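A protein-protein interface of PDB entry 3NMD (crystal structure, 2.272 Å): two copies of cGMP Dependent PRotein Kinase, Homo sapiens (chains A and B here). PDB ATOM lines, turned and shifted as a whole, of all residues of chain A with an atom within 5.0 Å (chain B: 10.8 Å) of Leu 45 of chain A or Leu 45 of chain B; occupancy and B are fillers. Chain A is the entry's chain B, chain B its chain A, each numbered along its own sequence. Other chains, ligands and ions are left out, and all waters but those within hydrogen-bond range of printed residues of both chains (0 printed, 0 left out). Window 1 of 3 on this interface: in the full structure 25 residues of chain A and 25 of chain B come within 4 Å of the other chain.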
ATOM      1  N   LEU A  41     -17.214 -13.153 -12.130  1.00  0.00           N
ATOM      2  CA  LEU A  41     -17.031 -13.877 -10.873  1.00  0.00           C
ATOM      3  C   LEU A  41     -15.751 -13.437 -10.156  1.00  0.00           C
ATOM      4  O   LEU A  41     -15.741 -13.236  -8.942  1.00  0.00           O
ATOM      5  CB  LEU A  41     -17.029 -15.382 -11.127  1.00  0.00           C
ATOM      6  CG  LEU A  41     -16.693 -16.303  -9.953  1.00  0.00           C
ATOM      7  CD1 LEU A  41     -17.587 -16.018  -8.757  1.00  0.00           C
ATOM      8  CD2 LEU A  41     -16.805 -17.762 -10.375  1.00  0.00           C
ATOM      9  N   ILE A  42     -14.682 -13.271 -10.921  1.00  0.00           N
ATOM     10  CA  ILE A  42     -13.401 -12.843 -10.372  1.00  0.00           C
ATOM     11  C   ILE A  42     -13.496 -11.462  -9.720  1.00  0.00           C
ATOM     12  O   ILE A  42     -12.912 -11.215  -8.657  1.00  0.00           O
ATOM     13  CB  ILE A  42     -12.312 -12.866 -11.464  1.00  0.00           C
ATOM     14  CG1 ILE A  42     -11.921 -14.313 -11.778  1.00  0.00           C
ATOM     15  CG2 ILE A  42     -11.092 -12.055 -11.043  1.00  0.00           C
ATOM     16  CD1 ILE A  42     -11.026 -14.465 -13.009  1.00  0.00           C
ATOM     17  N   ASP A  43     -14.243 -10.566 -10.354  1.00  0.00           N
ATOM     18  CA  ASP A  43     -14.445  -9.235  -9.807  1.00  0.00           C
ATOM     19  C   ASP A  43     -15.169  -9.324  -8.472  1.00  0.00           C
ATOM     20  O   ASP A  43     -14.843  -8.604  -7.527  1.00  0.00           O
ATOM     21  CB  ASP A  43     -15.248  -8.366 -10.778  1.00  0.00           C
ATOM     22  CG  ASP A  43     -14.457  -7.993 -12.015  1.00  0.00           C
ATOM     23  OD1 ASP A  43     -14.978  -7.211 -12.840  1.00  0.00           O
ATOM     24  OD2 ASP A  43     -13.313  -8.481 -12.161  1.00  0.00           O
ATOM     25  N   GLU A  44     -16.160 -10.206  -8.409  1.00  0.00           N
ATOM     26  CA  GLU A  44     -16.930 -10.404  -7.188  1.00  0.00           C
ATOM     27  C   GLU A  44     -16.046 -10.980  -6.091  1.00  0.00           C
ATOM     28  O   GLU A  44     -16.035 -10.485  -4.966  1.00  0.00           O
ATOM     29  CB  GLU A  44     -18.115 -11.331  -7.450  1.00  0.00           C
ATOM     30  CG  GLU A  44     -18.625 -12.041  -6.202  1.00  0.00           C
ATOM     31  CD  GLU A  44     -19.553 -13.205  -6.519  1.00  0.00           C
ATOM     32  OE1 GLU A  44     -20.400 -13.061  -7.430  1.00  0.00           O
ATOM     33  OE2 GLU A  44     -19.437 -14.261  -5.855  1.00  0.00           O
ATOM     34  N   LEU A  45     -15.303 -12.030  -6.430  1.00  0.00           N
ATOM     35  CA  LEU A  45     -14.439 -12.692  -5.469  1.00  0.00           C
ATOM     36  C   LEU A  45     -13.414 -11.725  -4.912  1.00  0.00           C
ATOM     37  O   LEU A  45     -13.157 -11.706  -3.707  1.00  0.00           O
ATOM     38  CB  LEU A  45     -13.738 -13.892  -6.105  1.00  0.00           C
ATOM     39  CG  LEU A  45     -14.663 -15.051  -6.444  1.00  0.00           C
ATOM     40  CD1 LEU A  45     -13.858 -16.255  -6.917  1.00  0.00           C
ATOM     41  CD2 LEU A  45     -15.532 -15.401  -5.235  1.00  0.00           C
ATOM     42  N   GLU A  46     -12.837 -10.914  -5.790  1.00  0.00           N
ATOM     43  CA  GLU A  46     -11.820  -9.969  -5.371  1.00  0.00           C
ATOM     44  C   GLU A  46     -12.384  -8.892  -4.454  1.00  0.00           C
ATOM     45  O   GLU A  46     -11.724  -8.477  -3.501  1.00  0.00           O
ATOM     46  CB  GLU A  46     -11.143  -9.335  -6.584  1.00  0.00           C
ATOM     47  CG  GLU A  46     -10.199 -10.282  -7.305  1.00  0.00           C
ATOM     48  CD  GLU A  46      -9.532  -9.647  -8.510  1.00  0.00           C
ATOM     49  OE1 GLU A  46     -10.050  -8.624  -9.015  1.00  0.00           O
ATOM     50  OE2 GLU A  46      -8.491 -10.176  -8.957  1.00  0.00           O
ATOM     51  N   LEU A  47     -13.595  -8.430  -4.753  1.00  0.00           N
ATOM     52  CA  LEU A  47     -14.245  -7.439  -3.910  1.00  0.00           C
ATOM     53  C   LEU A  47     -14.485  -8.044  -2.534  1.00  0.00           C
ATOM     54  O   LEU A  47     -14.275  -7.389  -1.510  1.00  0.00           O
ATOM     55  CB  LEU A  47     -15.560  -6.964  -4.536  1.00  0.00           C
ATOM     56  CG  LEU A  47     -16.515  -6.120  -3.677  1.00  0.00           C
ATOM     57  CD1 LEU A  47     -15.827  -4.905  -3.060  1.00  0.00           C
ATOM     58  CD2 LEU A  47     -17.731  -5.685  -4.490  1.00  0.00           C
ATOM     59  N   GLU A  48     -14.905  -9.306  -2.528  1.00  0.00           N
ATOM     60  CA  GLU A  48     -15.170 -10.044  -1.299  1.00  0.00           C
ATOM     61  C   GLU A  48     -13.939 -10.155  -0.421  1.00  0.00           C
ATOM     62  O   GLU A  48     -14.024  -9.972   0.793  1.00  0.00           O
ATOM     63  CB  GLU A  48     -15.678 -11.456  -1.606  1.00  0.00           C
ATOM     64  CG  GLU A  48     -17.186 -11.597  -1.711  1.00  0.00           C
ATOM     65  CD  GLU A  48     -17.649 -13.042  -1.539  1.00  0.00           C
ATOM     66  OE1 GLU A  48     -17.071 -13.762  -0.691  1.00  0.00           O
ATOM     67  OE2 GLU A  48     -18.595 -13.454  -2.248  1.00  0.00           O
ATOM     68  N   LEU A  49     -12.795 -10.476  -1.017  1.00  0.00           N
ATOM     69  CA  LEU A  49     -11.609 -10.667  -0.196  1.00  0.00           C
ATOM     70  C   LEU A  49     -11.054  -9.346   0.305  1.00  0.00           C
ATOM     71  O   LEU A  49     -10.462  -9.292   1.380  1.00  0.00           O
ATOM     72  CB  LEU A  49     -10.541 -11.529  -0.883  1.00  0.00           C
ATOM     73  CG  LEU A  49      -9.970 -11.184  -2.249  1.00  0.00           C
ATOM     74  CD1 LEU A  49      -9.090  -9.944  -2.178  1.00  0.00           C
ATOM     75  CD2 LEU A  49      -9.178 -12.381  -2.752  1.00  0.00           C
ATOM     76  N   GLN B  37      -6.452 -20.045 -17.316  1.00  0.00           N
ATOM     77  CA  GLN B  37      -5.814 -19.112 -16.393  1.00  0.00           C
ATOM     78  C   GLN B  37      -6.858 -18.514 -15.444  1.00  0.00           C
ATOM     79  O   GLN B  37      -6.649 -18.458 -14.238  1.00  0.00           O
ATOM     80  CB  GLN B  37      -5.064 -18.013 -17.147  1.00  0.00           C
ATOM     81  CG  GLN B  37      -3.849 -18.511 -17.923  1.00  0.00           C
ATOM     82  CD  GLN B  37      -3.398 -17.537 -19.003  1.00  0.00           C
ATOM     83  OE1 GLN B  37      -3.936 -16.436 -19.131  1.00  0.00           O
ATOM     84  NE2 GLN B  37      -2.408 -17.944 -19.791  1.00  0.00           N
ATOM     85  N   ARG B  38      -7.989 -18.085 -15.993  1.00  0.00           N
ATOM     86  CA  ARG B  38      -9.077 -17.568 -15.167  1.00  0.00           C
ATOM     87  C   ARG B  38      -9.488 -18.576 -14.095  1.00  0.00           C
ATOM     88  O   ARG B  38      -9.655 -18.229 -12.923  1.00  0.00           O
ATOM     89  CB  ARG B  38     -10.281 -17.181 -16.032  1.00  0.00           C
ATOM     90  CG  ARG B  38     -10.465 -15.679 -16.238  1.00  0.00           C
ATOM     91  CD  ARG B  38      -9.319 -15.022 -16.988  1.00  0.00           C
ATOM     92  NE  ARG B  38      -9.759 -13.796 -17.649  1.00  0.00           N
ATOM     93  CZ  ARG B  38      -9.069 -13.152 -18.589  1.00  0.00           C
ATOM     94  NH1 ARG B  38      -7.890 -13.610 -18.985  1.00  0.00           N
ATOM     95  NH2 ARG B  38      -9.565 -12.049 -19.137  1.00  0.00           N
ATOM     96  N   ASP B  39      -9.639 -19.829 -14.502  1.00  0.00           N
ATOM     97  CA  ASP B  39     -10.033 -20.885 -13.581  1.00  0.00           C
ATOM     98  C   ASP B  39      -8.988 -21.110 -12.489  1.00  0.00           C
ATOM     99  O   ASP B  39      -9.333 -21.367 -11.334  1.00  0.00           O
ATOM    100  CB  ASP B  39     -10.313 -22.183 -14.344  1.00  0.00           C
ATOM    101  CG  ASP B  39     -11.688 -22.192 -14.992  1.00  0.00           C
ATOM    102  OD1 ASP B  39     -12.521 -21.334 -14.629  1.00  0.00           O
ATOM    103  OD2 ASP B  39     -11.940 -23.061 -15.858  1.00  0.00           O
ATOM    104  N   ALA B  40      -7.713 -21.005 -12.851  1.00  0.00           N
ATOM    105  CA  ALA B  40      -6.648 -21.163 -11.863  1.00  0.00           C
ATOM    106  C   ALA B  40      -6.691 -20.015 -10.849  1.00  0.00           C
ATOM    107  O   ALA B  40      -6.495 -20.215  -9.650  1.00  0.00           O
ATOM    108  CB  ALA B  40      -5.273 -21.245 -12.543  1.00  0.00           C
ATOM    109  N   LEU B  41      -6.953 -18.810 -11.341  1.00  0.00           N
ATOM    110  CA  LEU B  41      -7.052 -17.642 -10.472  1.00  0.00           C
ATOM    111  C   LEU B  41      -8.221 -17.795  -9.495  1.00  0.00           C
ATOM    112  O   LEU B  41      -8.077 -17.558  -8.296  1.00  0.00           O
ATOM    113  CB  LEU B  41      -7.203 -16.371 -11.313  1.00  0.00           C
ATOM    114  CG  LEU B  41      -7.472 -15.051 -10.577  1.00  0.00           C
ATOM    115  CD1 LEU B  41      -6.564 -14.879  -9.351  1.00  0.00           C
ATOM    116  CD2 LEU B  41      -7.313 -13.884 -11.538  1.00  0.00           C
ATOM    117  N   ILE B  42      -9.372 -18.207 -10.017  1.00  0.00           N
ATOM    118  CA  ILE B  42     -10.554 -18.435  -9.191  1.00  0.00           C
ATOM    119  C   ILE B  42     -10.265 -19.411  -8.054  1.00  0.00           C
ATOM    120  O   ILE B  42     -10.603 -19.140  -6.905  1.00  0.00           O
ATOM    121  CB  ILE B  42     -11.752 -18.912 -10.035  1.00  0.00           C
ATOM    122  CG1 ILE B  42     -12.244 -17.762 -10.923  1.00  0.00           C
ATOM    123  CG2 ILE B  42     -12.871 -19.401  -9.144  1.00  0.00           C
ATOM    124  CD1 ILE B  42     -13.270 -18.152 -11.957  1.00  0.00           C
ATOM    125  N   ASP B  43      -9.623 -20.532  -8.374  1.00  0.00           N
ATOM    126  CA  ASP B  43      -9.225 -21.506  -7.358  1.00  0.00           C
ATOM    127  C   ASP B  43      -8.368 -20.887  -6.260  1.00  0.00           C
ATOM    128  O   ASP B  43      -8.571 -21.169  -5.082  1.00  0.00           O
ATOM    129  CB  ASP B  43      -8.471 -22.676  -7.989  1.00  0.00           C
ATOM    130  CG  ASP B  43      -9.376 -23.584  -8.786  1.00  0.00           C
ATOM    131  OD1 ASP B  43     -10.613 -23.466  -8.628  1.00  0.00           O
ATOM    132  OD2 ASP B  43      -8.853 -24.413  -9.566  1.00  0.00           O
ATOM    133  N   GLU B  44      -7.402 -20.060  -6.649  1.00  0.00           N
ATOM    134  CA  GLU B  44      -6.539 -19.401  -5.675  1.00  0.00           C
ATOM    135  C   GLU B  44      -7.330 -18.432  -4.808  1.00  0.00           C
ATOM    136  O   GLU B  44      -7.095 -18.324  -3.602  1.00  0.00           O
ATOM    137  CB  GLU B  44      -5.405 -18.663  -6.378  1.00  0.00           C
ATOM    138  CG  GLU B  44      -4.370 -19.585  -6.999  1.00  0.00           C
ATOM    139  CD  GLU B  44      -3.241 -18.823  -7.663  1.00  0.00           C
ATOM    140  OE1 GLU B  44      -3.373 -17.588  -7.807  1.00  0.00           O
ATOM    141  OE2 GLU B  44      -2.228 -19.453  -8.040  1.00  0.00           O
ATOM    142  N   LEU B  45      -8.272 -17.737  -5.433  1.00  0.00           N
ATOM    143  CA  LEU B  45      -9.099 -16.757  -4.741  1.00  0.00           C
ATOM    144  C   LEU B  45     -10.008 -17.412  -3.721  1.00  0.00           C
ATOM    145  O   LEU B  45     -10.142 -16.934  -2.593  1.00  0.00           O
ATOM    146  CB  LEU B  45      -9.958 -15.986  -5.745  1.00  0.00           C
ATOM    147  CG  LEU B  45      -9.223 -14.998  -6.645  1.00  0.00           C
ATOM    148  CD1 LEU B  45     -10.192 -14.326  -7.606  1.00  0.00           C
ATOM    149  CD2 LEU B  45      -8.510 -13.967  -5.791  1.00  0.00           C
ATOM    150  N   GLU B  46     -10.648 -18.497  -4.131  1.00  0.00           N
ATOM    151  CA  GLU B  46     -11.559 -19.213  -3.257  1.00  0.00           C
ATOM    152  C   GLU B  46     -10.809 -19.856  -2.094  1.00  0.00           C
ATOM    153  O   GLU B  46     -11.342 -19.994  -0.988  1.00  0.00           O
ATOM    154  CB  GLU B  46     -12.341 -20.251  -4.052  1.00  0.00           C
ATOM    155  CG  GLU B  46     -13.405 -19.632  -4.933  1.00  0.00           C
ATOM    156  CD  GLU B  46     -14.199 -20.662  -5.701  1.00  0.00           C
ATOM    157  OE1 GLU B  46     -13.747 -21.826  -5.777  1.00  0.00           O
ATOM    158  OE2 GLU B  46     -15.275 -20.303  -6.233  1.00  0.00           O
ATOM    159  N   LEU B  47      -9.565 -20.236  -2.355  1.00  0.00           N
ATOM    160  CA  LEU B  47      -8.696 -20.757  -1.313  1.00  0.00           C
ATOM    161  C   LEU B  47      -8.387 -19.646  -0.319  1.00  0.00           C
ATOM    162  O   LEU B  47      -8.469 -19.840   0.892  1.00  0.00           O
ATOM    163  CB  LEU B  47      -7.399 -21.286  -1.927  1.00  0.00           C
ATOM    164  CG  LEU B  47      -6.547 -22.194  -1.053  1.00  0.00           C
ATOM    165  CD1 LEU B  47      -7.249 -23.529  -0.898  1.00  0.00           C
ATOM    166  CD2 LEU B  47      -5.167 -22.377  -1.667  1.00  0.00           C
ATOM    167  N   GLU B  48      -8.038 -18.476  -0.845  1.00  0.00           N
ATOM    168  CA  GLU B  48      -7.711 -17.325  -0.010  1.00  0.00           C
ATOM    169  C   GLU B  48      -8.910 -16.906   0.843  1.00  0.00           C
ATOM    170  O   GLU B  48      -8.754 -16.512   2.000  1.00  0.00           O
ATOM    171  CB  GLU B  48      -7.230 -16.153  -0.868  1.00  0.00           C
ATOM    172  CG  GLU B  48      -6.703 -14.973  -0.066  1.00  0.00           C
ATOM    173  CD  GLU B  48      -6.256 -13.815  -0.943  1.00  0.00           C
ATOM    174  OE1 GLU B  48      -5.930 -12.740  -0.391  1.00  0.00           O
ATOM    175  N   LEU B  49     -10.104 -17.011   0.268  1.00  0.00           N
ATOM    176  CA  LEU B  49     -11.330 -16.646   0.970  1.00  0.00           C
ATOM    177  C   LEU B  49     -11.590 -17.549   2.166  1.00  0.00           C
ATOM    178  O   LEU B  49     -11.953 -17.078   3.242  1.00  0.00           O
ATOM    179  CB  LEU B  49     -12.533 -16.678   0.028  1.00  0.00           C
ATOM    180  CG  LEU B  49     -12.624 -15.492  -0.928  1.00  0.00           C
ATOM    181  CD1 LEU B  49     -13.871 -15.592  -1.788  1.00  0.00           C
ATOM    182  CD2 LEU B  49     -12.608 -14.192  -0.145  1.00  0.00           C
ATOM    183  N   ASP B  50     -11.412 -18.850   1.970  1.00  0.00           N
ATOM    184  CA  ASP B  50     -11.627 -19.803   3.047  1.00  0.00           C
ATOM    185  C   ASP B  50     -10.674 -19.543   4.210  1.00  0.00           C
ATOM    186  O   ASP B  50     -11.048 -19.693   5.368  1.00  0.00           O
ATOM    187  CB  ASP B  50     -11.494 -21.236   2.535  1.00  0.00           C
ATOM    188  CG  ASP B  50     -12.603 -21.608   1.566  1.00  0.00           C
ATOM    189  OD1 ASP B  50     -13.655 -20.933   1.582  1.00  0.00           O
ATOM    190  OD2 ASP B  50     -12.426 -22.572   0.792  1.00  0.00           O
ATOM    191  N   GLN B  51      -9.450 -19.133   3.895  1.00  0.00           N
ATOM    192  CA  GLN B  51      -8.458 -18.839   4.923  1.00  0.00           C
ATOM    193  C   GLN B  51      -8.866 -17.611   5.733  1.00  0.00           C
ATOM    194  O   GLN B  51      -8.798 -17.613   6.958  1.00  0.00           O
ATOM    195  CB  GLN B  51      -7.075 -18.643   4.295  1.00  0.00           C
ATOM    196  CG  GLN B  51      -6.589 -19.854   3.498  1.00  0.00           C
ATOM    197  CD  GLN B  51      -5.417 -19.541   2.580  1.00  0.00           C
ATOM    198  OE1 GLN B  51      -4.854 -18.445   2.618  1.00  0.00           O
ATOM    199  NE2 GLN B  51      -5.045 -20.507   1.747  1.00  0.00           N
ATOM    200  N   LYS B  52      -9.305 -16.570   5.037  1.00  0.00           N
ATOM    201  CA  LYS B  52      -9.751 -15.347   5.690  1.00  0.00           C
ATOM    202  C   LYS B  52     -11.011 -15.595   6.501  1.00  0.00           C
ATOM    203  O   LYS B  52     -11.200 -14.998   7.557  1.00  0.00           O
ATOM    204  CB  LYS B  52     -10.005 -14.251   4.662  1.00  0.00           C
ATOM    205  CG  LYS B  52      -8.768 -13.832   3.904  1.00  0.00           C
ATOM    206  CD  LYS B  52      -8.997 -12.510   3.185  1.00  0.00           C
ATOM    207  CE  LYS B  52      -7.760 -12.105   2.396  1.00  0.00           C
ATOM    208  NZ  LYS B  52      -6.520 -12.294   3.201  1.00  0.00           N
ATOM    209  N   ASP B  53     -11.865 -16.481   6.005  1.00  0.00           N
ATOM    210  CA  ASP B  53     -13.070 -16.867   6.724  1.00  0.00           C
ATOM    211  C   ASP B  53     -12.742 -17.521   8.060  1.00  0.00           C
ATOM    212  O   ASP B  53     -13.388 -17.244   9.077  1.00  0.00           O
ATOM    213  CB  ASP B  53     -13.917 -17.813   5.877  1.00  0.00           C
ATOM    214  CG  ASP B  53     -14.922 -17.079   5.018  1.00  0.00           C
ATOM    215  OD1 ASP B  53     -15.158 -15.879   5.282  1.00  0.00           O
ATOM    216  OD2 ASP B  53     -15.480 -17.699   4.089  1.00  0.00           O
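The side-chain carboxylate (OE1) of Glu 48 of chain B lies within salt-bridge range of the side-chain amino group (NZ) of Lys 52 of chain B (3.7 Å).
Ile 42 of chain B touches Leu 41 of chain A (CD1 to CD2, 3.9 Å).
Ile 42 of chain A touches Arg 38 of chain B (CD1 to CG, 3.5 Å).
Ile 42 of chain A touches Ile 42 of chain B (CG1 to CG1, 3.6 Å).
CG2 of Ile 42 of chain B touches CD1 of Leu 45 of chain A (3.98 Å).
Leu 45 of chain B touches Leu 45 of chain A.
Leu 45 of chain A touches Leu 49 of chain B (CD2 to CD1, 3.8 Å).
Glu 48 of chain A touches Leu 49 of chain B (OE1 to CD1, 3.8 Å).
Leu 45 of chain B touches Leu 49 of chain A (CD2 to CD2, 3.5 Å).
Leu 49 of chain A touches Glu 48 of chain B (CD2 to CD, 3.7 Å).
Leu 49 of chain A touches Leu 49 of chain B (CB to CD2, 3.5 Å).
Leu 41 of chain A touches one residue of chain B.
Of chain B, only Arg 38 and Ile 42 come within 4 Å of Ile 42 of chain A.
No residue of chain B comes within 4 Å of Glu 44 of chain A.
Leu 45 of chain A touches four residues of chain B.
Of chain B, only Leu 49 comes within 4 Å of Glu 48 of chain A.
Of the printed residues of chain A, Arg 38 of chain B touches Ile 42.
Of chain A, only Leu 45 and Leu 49 come within 4 Å of Leu 45 of chain B.
Of the printed residues of chain A, Leu 49 of chain B touches Leu 45 (3.8 Å), Glu 48 (3.8 Å) and Leu 49 (3.5 Å).
Printed residues of chain A within 4 Å of Lys 52 of chain B: Leu 49 (3.97 Å).
The nearest residue of chain B that does not touch Leu 45 of chain A is Leu 41 of chain B (6.1 Å).
Of the 9 printed residues of chain A, 5 touch a printed residue of chain B.
Of the 17 printed residues of chain B, 7 touch a printed residue of chain A.
Printed residues of chain B that touch a printed residue of chain A: Arg 38, Ile 42, Leu 45, Glu 46, Glu 48, Leu 49 and Lys 52.
Hydrophobic or aromatic side chains of chain B within 4 Å of the printed part of chain A: Ile 42, Leu 45 and Leu 49.
Among the printed residues, 12 pairs touch across the chains.
Among the printed residues, no Asp or Glu carboxylate lies within 4 Å of a Lys or Arg side-chain nitrogen of the other chain.
Leu 41 of chain A touches Ile 42 of chain B, but with the chains exchanged Ile 42 of chain A does not touch Leu 41 of chain B (4.04 Å).
Leu 45 of chain A touches Ile 42 of chain B, but with the chains exchanged Ile 42 of chain A does not touch Leu 45 of chain B (4.2 Å).
Glu 48 of chain A touches Leu 49 of chain B, and with the chains exchanged Leu 49 of chain A touches Glu 48 of chain B.
Leu 49 of chain B touches its own counterpart, Leu 49 of chain A.
9 positions are printed for both chains.
Of the 12 pairs that touch across the chains among the printed residues, 7 have their exchanged pair printed and touching as well.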
